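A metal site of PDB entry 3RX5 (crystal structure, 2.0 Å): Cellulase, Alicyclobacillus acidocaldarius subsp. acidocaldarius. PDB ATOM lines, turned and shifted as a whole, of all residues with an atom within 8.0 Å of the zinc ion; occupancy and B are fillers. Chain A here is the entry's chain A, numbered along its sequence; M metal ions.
A ring nitrogen (NE2) of His 122 is in hydrogen-bond range of the side-chain carboxylate (OD2) of Asp 231.
The side-chain sulfur of Cys 104 sits close to the side-chain amino group of Lys 149 (3.8 Å).
O of Gly 140 sits at hydrogen-bond distance from N of Cys 104, 3.0 Å away.
N of His 142 sits at hydrogen-bond distance from O of Gln 102, at 2.8 Å.
O of Cys 121 is in hydrogen-bond range of N of Gly 105 (3.0 Å).
Within 4 Å of the zinc ion: Cys 104, Cys 121, His 122 and His 142.
The nearest printed residue that does not touch the zinc ion is Gly 105 (4.03 Å).
The zinc ion is bound by NE2 of His 142 (2.1 Å), ND1 of His 122 (2.1 Å), SG of Cys 104 (2.3 Å) and SG of Cys 121 (2.3 Å).
The zinc ion has four donor atoms within binding distance.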
ATOM      1  N   GLN A 102       8.649  27.440  26.664  1.00  0.00           N
ATOM      2  CA  GLN A 102       8.918  26.492  25.570  1.00  0.00           C
ATOM      3  C   GLN A 102      10.256  26.778  24.868  1.00  0.00           C
ATOM      4  O   GLN A 102      10.637  26.009  23.987  1.00  0.00           O
ATOM      5  CB  GLN A 102       7.787  26.510  24.518  1.00  0.00           C
ATOM      6  CG  GLN A 102       6.454  25.954  24.974  1.00  0.00           C
ATOM      7  CD  GLN A 102       6.502  24.470  25.255  1.00  0.00           C
ATOM      8  OE1 GLN A 102       6.785  24.071  26.385  1.00  0.00           O
ATOM      9  NE2 GLN A 102       6.215  23.637  24.242  1.00  0.00           N
ATOM     10  N   LEU A 103      10.935  27.876  25.216  1.00  0.00           N
ATOM     11  CA  LEU A 103      12.196  28.243  24.560  1.00  0.00           C
ATOM     12  C   LEU A 103      13.231  27.134  24.557  1.00  0.00           C
ATOM     13  O   LEU A 103      13.448  26.478  25.580  1.00  0.00           O
ATOM     14  CB  LEU A 103      12.810  29.554  25.107  1.00  0.00           C
ATOM     15  CG  LEU A 103      12.149  30.867  24.673  1.00  0.00           C
ATOM     16  CD1 LEU A 103      12.555  32.004  25.585  1.00  0.00           C
ATOM     17  CD2 LEU A 103      12.458  31.202  23.190  1.00  0.00           C
ATOM     18  N   CYS A 104      13.824  26.900  23.378  1.00  0.00           N
ATOM     19  CA  CYS A 104      14.851  25.871  23.149  1.00  0.00           C
ATOM     20  C   CYS A 104      16.233  26.554  23.036  1.00  0.00           C
ATOM     21  O   CYS A 104      16.309  27.618  22.449  1.00  0.00           O
ATOM     22  CB  CYS A 104      14.514  25.129  21.869  1.00  0.00           C
ATOM     23  SG  CYS A 104      15.582  23.709  21.528  1.00  0.00           S
ATOM     24  N   GLY A 105      17.286  25.909  23.552  1.00  0.00           N
ATOM     25  CA  GLY A 105      18.652  26.409  23.435  1.00  0.00           C
ATOM     26  C   GLY A 105      18.970  27.659  24.237  1.00  0.00           C
ATOM     27  O   GLY A 105      19.933  28.367  23.917  1.00  0.00           O
ATOM     28  N   VAL A 106      18.174  27.905  25.277  1.00  0.00           N
ATOM     29  CA  VAL A 106      18.200  29.122  26.093  1.00  0.00           C
ATOM     30  C   VAL A 106      18.134  28.778  27.572  1.00  0.00           C
ATOM     31  O   VAL A 106      17.268  27.997  28.001  1.00  0.00           O
ATOM     32  CB  VAL A 106      16.994  30.035  25.652  1.00  0.00           C
ATOM     33  CG1 VAL A 106      16.660  31.130  26.670  1.00  0.00           C
ATOM     34  CG2 VAL A 106      17.216  30.641  24.270  1.00  0.00           C
ATOM     35  N   HIS A 118      15.409  25.683  33.729  1.00  0.00           N
ATOM     36  CA  HIS A 118      16.263  24.651  33.147  1.00  0.00           C
ATOM     37  C   HIS A 118      17.366  25.300  32.325  1.00  0.00           C
ATOM     38  O   HIS A 118      17.254  26.481  31.958  1.00  0.00           O
ATOM     39  CB  HIS A 118      15.461  23.595  32.330  1.00  0.00           C
ATOM     40  CG  HIS A 118      14.876  24.075  31.043  1.00  0.00           C
ATOM     41  ND1 HIS A 118      15.672  24.283  29.921  1.00  0.00           N
ATOM     42  CD2 HIS A 118      13.581  24.308  30.712  1.00  0.00           C
ATOM     43  CE1 HIS A 118      14.835  24.645  28.951  1.00  0.00           C
ATOM     44  NE2 HIS A 118      13.571  24.685  29.392  1.00  0.00           N
ATOM     45  N   GLY A 119      18.418  24.530  32.050  1.00  0.00           N
ATOM     46  CA  GLY A 119      19.552  24.988  31.243  1.00  0.00           C
ATOM     47  C   GLY A 119      19.269  24.919  29.756  1.00  0.00           C
ATOM     48  O   GLY A 119      18.247  24.374  29.348  1.00  0.00           O
ATOM     49  N   ALA A 120      20.184  25.469  28.930  1.00  0.00           N
ATOM     50  CA  ALA A 120      20.072  25.476  27.462  1.00  0.00           C
ATOM     51  C   ALA A 120      20.005  24.045  26.933  1.00  0.00           C
ATOM     52  O   ALA A 120      20.842  23.207  27.284  1.00  0.00           O
ATOM     53  CB  ALA A 120      21.233  26.225  26.842  1.00  0.00           C
ATOM     54  N   CYS A 121      18.997  23.747  26.126  1.00  0.00           N
ATOM     55  CA  CYS A 121      18.771  22.396  25.618  1.00  0.00           C
ATOM     56  C   CYS A 121      18.948  22.353  24.110  1.00  0.00           C
ATOM     57  O   CYS A 121      18.875  23.399  23.466  1.00  0.00           O
ATOM     58  CB  CYS A 121      17.364  21.960  26.006  1.00  0.00           C
ATOM     59  SG  CYS A 121      16.063  23.063  25.405  1.00  0.00           S
ATOM     60  N   HIS A 122      19.194  21.140  23.536  1.00  0.00           N
ATOM     61  CA  HIS A 122      19.291  20.944  22.082  1.00  0.00           C
ATOM     62  C   HIS A 122      20.222  21.954  21.392  1.00  0.00           C
ATOM     63  O   HIS A 122      19.861  22.549  20.363  1.00  0.00           O
ATOM     64  CB  HIS A 122      17.864  21.013  21.447  1.00  0.00           C
ATOM     65  CG  HIS A 122      16.916  20.053  22.066  1.00  0.00           C
ATOM     66  ND1 HIS A 122      15.894  20.484  22.895  1.00  0.00           N
ATOM     67  CD2 HIS A 122      16.890  18.707  22.001  1.00  0.00           C
ATOM     68  CE1 HIS A 122      15.279  19.386  23.301  1.00  0.00           C
ATOM     69  NE2 HIS A 122      15.851  18.294  22.782  1.00  0.00           N
ATOM     70  N   THR A 123      21.434  22.132  21.936  1.00  0.00           N
ATOM     71  CA  THR A 123      22.383  23.113  21.423  1.00  0.00           C
ATOM     72  C   THR A 123      23.230  22.657  20.256  1.00  0.00           C
ATOM     73  O   THR A 123      23.875  23.486  19.609  1.00  0.00           O
ATOM     74  CB  THR A 123      23.201  23.734  22.548  1.00  0.00           C
ATOM     75  OG1 THR A 123      23.817  22.679  23.286  1.00  0.00           O
ATOM     76  CG2 THR A 123      22.356  24.625  23.449  1.00  0.00           C
ATOM     77  N   GLY A 139      17.300  27.841  19.074  1.00  0.00           N
ATOM     78  CA  GLY A 139      16.281  28.790  19.474  1.00  0.00           C
ATOM     79  C   GLY A 139      14.892  28.379  19.061  1.00  0.00           C
ATOM     80  O   GLY A 139      14.649  27.235  18.679  1.00  0.00           O
ATOM     81  N   GLY A 140      13.973  29.323  19.130  1.00  0.00           N
ATOM     82  CA  GLY A 140      12.584  29.049  18.822  1.00  0.00           C
ATOM     83  C   GLY A 140      11.963  28.248  19.948  1.00  0.00           C
ATOM     84  O   GLY A 140      12.497  28.205  21.063  1.00  0.00           O
ATOM     85  N   TRP A 141      10.828  27.612  19.667  1.00  0.00           N
ATOM     86  CA  TRP A 141      10.057  26.934  20.707  1.00  0.00           C
ATOM     87  C   TRP A 141       9.938  25.454  20.506  1.00  0.00           C
ATOM     88  O   TRP A 141       9.731  25.006  19.373  1.00  0.00           O
ATOM     89  CB  TRP A 141       8.601  27.518  20.755  1.00  0.00           C
ATOM     90  CG  TRP A 141       8.500  29.008  20.937  1.00  0.00           C
ATOM     91  CD1 TRP A 141       9.187  29.776  21.826  1.00  0.00           C
ATOM     92  CD2 TRP A 141       7.583  29.897  20.264  1.00  0.00           C
ATOM     93  NE1 TRP A 141       8.796  31.091  21.711  1.00  0.00           N
ATOM     94  CE2 TRP A 141       7.839  31.197  20.742  1.00  0.00           C
ATOM     95  CE3 TRP A 141       6.628  29.728  19.233  1.00  0.00           C
ATOM     96  CZ2 TRP A 141       7.121  32.326  20.284  1.00  0.00           C
ATOM     97  CZ3 TRP A 141       5.898  30.838  18.797  1.00  0.00           C
ATOM     98  CH2 TRP A 141       6.143  32.119  19.326  1.00  0.00           C
ATOM     99  N   HIS A 142       9.940  24.694  21.610  1.00  0.00           N
ATOM    100  CA  HIS A 142       9.566  23.282  21.556  1.00  0.00           C
ATOM    101  C   HIS A 142       8.066  23.373  21.185  1.00  0.00           C
ATOM    102  O   HIS A 142       7.334  24.234  21.700  1.00  0.00           O
ATOM    103  CB  HIS A 142       9.698  22.605  22.922  1.00  0.00           C
ATOM    104  CG  HIS A 142      11.089  22.575  23.467  1.00  0.00           C
ATOM    105  ND1 HIS A 142      11.336  22.858  24.798  1.00  0.00           N
ATOM    106  CD2 HIS A 142      12.266  22.371  22.826  1.00  0.00           C
ATOM    107  CE1 HIS A 142      12.651  22.755  24.950  1.00  0.00           C
ATOM    108  NE2 HIS A 142      13.258  22.459  23.806  1.00  0.00           N
ATOM    109  N   ASP A 146       6.415  17.560  23.325  1.00  0.00           N
ATOM    110  CA  ASP A 146       7.685  17.014  22.811  1.00  0.00           C
ATOM    111  C   ASP A 146       8.660  18.181  22.529  1.00  0.00           C
ATOM    112  O   ASP A 146       8.302  19.336  22.663  1.00  0.00           O
ATOM    113  CB  ASP A 146       7.434  16.183  21.556  1.00  0.00           C
ATOM    114  CG  ASP A 146       7.078  17.005  20.341  1.00  0.00           C
ATOM    115  OD1 ASP A 146       6.074  17.760  20.416  1.00  0.00           O
ATOM    116  OD2 ASP A 146       7.769  16.883  19.319  1.00  0.00           O
ATOM    117  N   TYR A 147       9.865  17.863  22.073  1.00  0.00           N
ATOM    118  CA  TYR A 147      10.891  18.850  21.839  1.00  0.00           C
ATOM    119  C   TYR A 147      11.159  19.230  20.400  1.00  0.00           C
ATOM    120  O   TYR A 147      12.021  20.075  20.147  1.00  0.00           O
ATOM    121  CB  TYR A 147      12.169  18.414  22.577  1.00  0.00           C
ATOM    122  CG  TYR A 147      11.961  18.242  24.067  1.00  0.00           C
ATOM    123  CD1 TYR A 147      11.394  19.264  24.842  1.00  0.00           C
ATOM    124  CD2 TYR A 147      12.378  17.084  24.724  1.00  0.00           C
ATOM    125  CE1 TYR A 147      11.205  19.105  26.218  1.00  0.00           C
ATOM    126  CE2 TYR A 147      12.225  16.935  26.106  1.00  0.00           C
ATOM    127  CZ  TYR A 147      11.645  17.949  26.853  1.00  0.00           C
ATOM    128  OH  TYR A 147      11.503  17.807  28.220  1.00  0.00           O
ATOM    129  N   GLY A 148      10.413  18.671  19.456  1.00  0.00           N
ATOM    130  CA  GLY A 148      10.581  19.015  18.043  1.00  0.00           C
ATOM    131  C   GLY A 148      10.174  20.451  17.731  1.00  0.00           C
ATOM    132  O   GLY A 148       9.353  21.035  18.450  1.00  0.00           O
ATOM    133  N   LYS A 149      10.743  21.011  16.666  1.00  0.00           N
ATOM    134  CA  LYS A 149      10.447  22.387  16.221  1.00  0.00           C
ATOM    135  C   LYS A 149      10.063  22.258  14.789  1.00  0.00           C
ATOM    136  O   LYS A 149      10.865  21.850  13.934  1.00  0.00           O
ATOM    137  CB  LYS A 149      11.662  23.327  16.425  1.00  0.00           C
ATOM    138  CG  LYS A 149      12.250  23.262  17.857  1.00  0.00           C
ATOM    139  CD  LYS A 149      13.301  24.336  18.145  1.00  0.00           C
ATOM    140  CE  LYS A 149      14.649  24.023  17.505  1.00  0.00           C
ATOM    141  NZ  LYS A 149      15.728  24.937  17.942  1.00  0.00           N
ATOM    142  N   PRO A 228      14.363  18.638  29.318  1.00  0.00           N
ATOM    143  CA  PRO A 228      14.850  19.177  28.031  1.00  0.00           C
ATOM    144  C   PRO A 228      16.367  19.061  27.820  1.00  0.00           C
ATOM    145  O   PRO A 228      16.792  18.715  26.727  1.00  0.00           O
ATOM    146  CB  PRO A 228      14.356  20.650  28.033  1.00  0.00           C
ATOM    147  CG  PRO A 228      13.910  20.932  29.417  1.00  0.00           C
ATOM    148  CD  PRO A 228      13.536  19.624  30.048  1.00  0.00           C
ATOM    149  N   GLU A 229      17.156  19.307  28.878  1.00  0.00           N
ATOM    150  CA  GLU A 229      18.617  19.259  28.818  1.00  0.00           C
ATOM    151  C   GLU A 229      19.228  17.854  28.859  1.00  0.00           C
ATOM    152  O   GLU A 229      20.435  17.707  28.621  1.00  0.00           O
ATOM    153  CB  GLU A 229      19.280  20.231  29.812  1.00  0.00           C
ATOM    154  CG  GLU A 229      19.013  19.933  31.278  1.00  0.00           C
ATOM    155  CD  GLU A 229      17.833  20.657  31.893  1.00  0.00           C
ATOM    156  OE1 GLU A 229      16.694  20.498  31.388  1.00  0.00           O
ATOM    157  OE2 GLU A 229      18.031  21.321  32.932  1.00  0.00           O
ATOM    158  N   ASP A 231      17.873  15.510  26.848  1.00  0.00           N
ATOM    159  CA  ASP A 231      17.524  14.982  25.538  1.00  0.00           C
ATOM    160  C   ASP A 231      18.704  15.180  24.576  1.00  0.00           C
ATOM    161  O   ASP A 231      18.792  16.183  23.847  1.00  0.00           O
ATOM    162  CB  ASP A 231      16.204  15.609  25.034  1.00  0.00           C
ATOM    163  CG  ASP A 231      15.687  15.005  23.747  1.00  0.00           C
ATOM    164  OD1 ASP A 231      15.978  13.813  23.490  1.00  0.00           O
ATOM    165  OD2 ASP A 231      15.012  15.725  22.979  1.00  0.00           O
ATOM    166  N   LEU A 235      20.084  15.705  16.444  1.00  0.00           N
ATOM    167  CA  LEU A 235      19.014  16.481  15.814  1.00  0.00           C
ATOM    168  C   LEU A 235      19.068  16.284  14.298  1.00  0.00           C
ATOM    169  O   LEU A 235      20.140  16.250  13.711  1.00  0.00           O
ATOM    170  CB  LEU A 235      19.142  17.974  16.162  1.00  0.00           C
ATOM    171  CG  LEU A 235      18.820  18.386  17.625  1.00  0.00           C
ATOM    172  CD1 LEU A 235      19.246  19.824  17.882  1.00  0.00           C
ATOM    173  CD2 LEU A 235      17.324  18.199  17.979  1.00  0.00           C
HETATM  174 ZN    ZN M   1      15.272  22.428  23.373  1.00  0.00          ZN
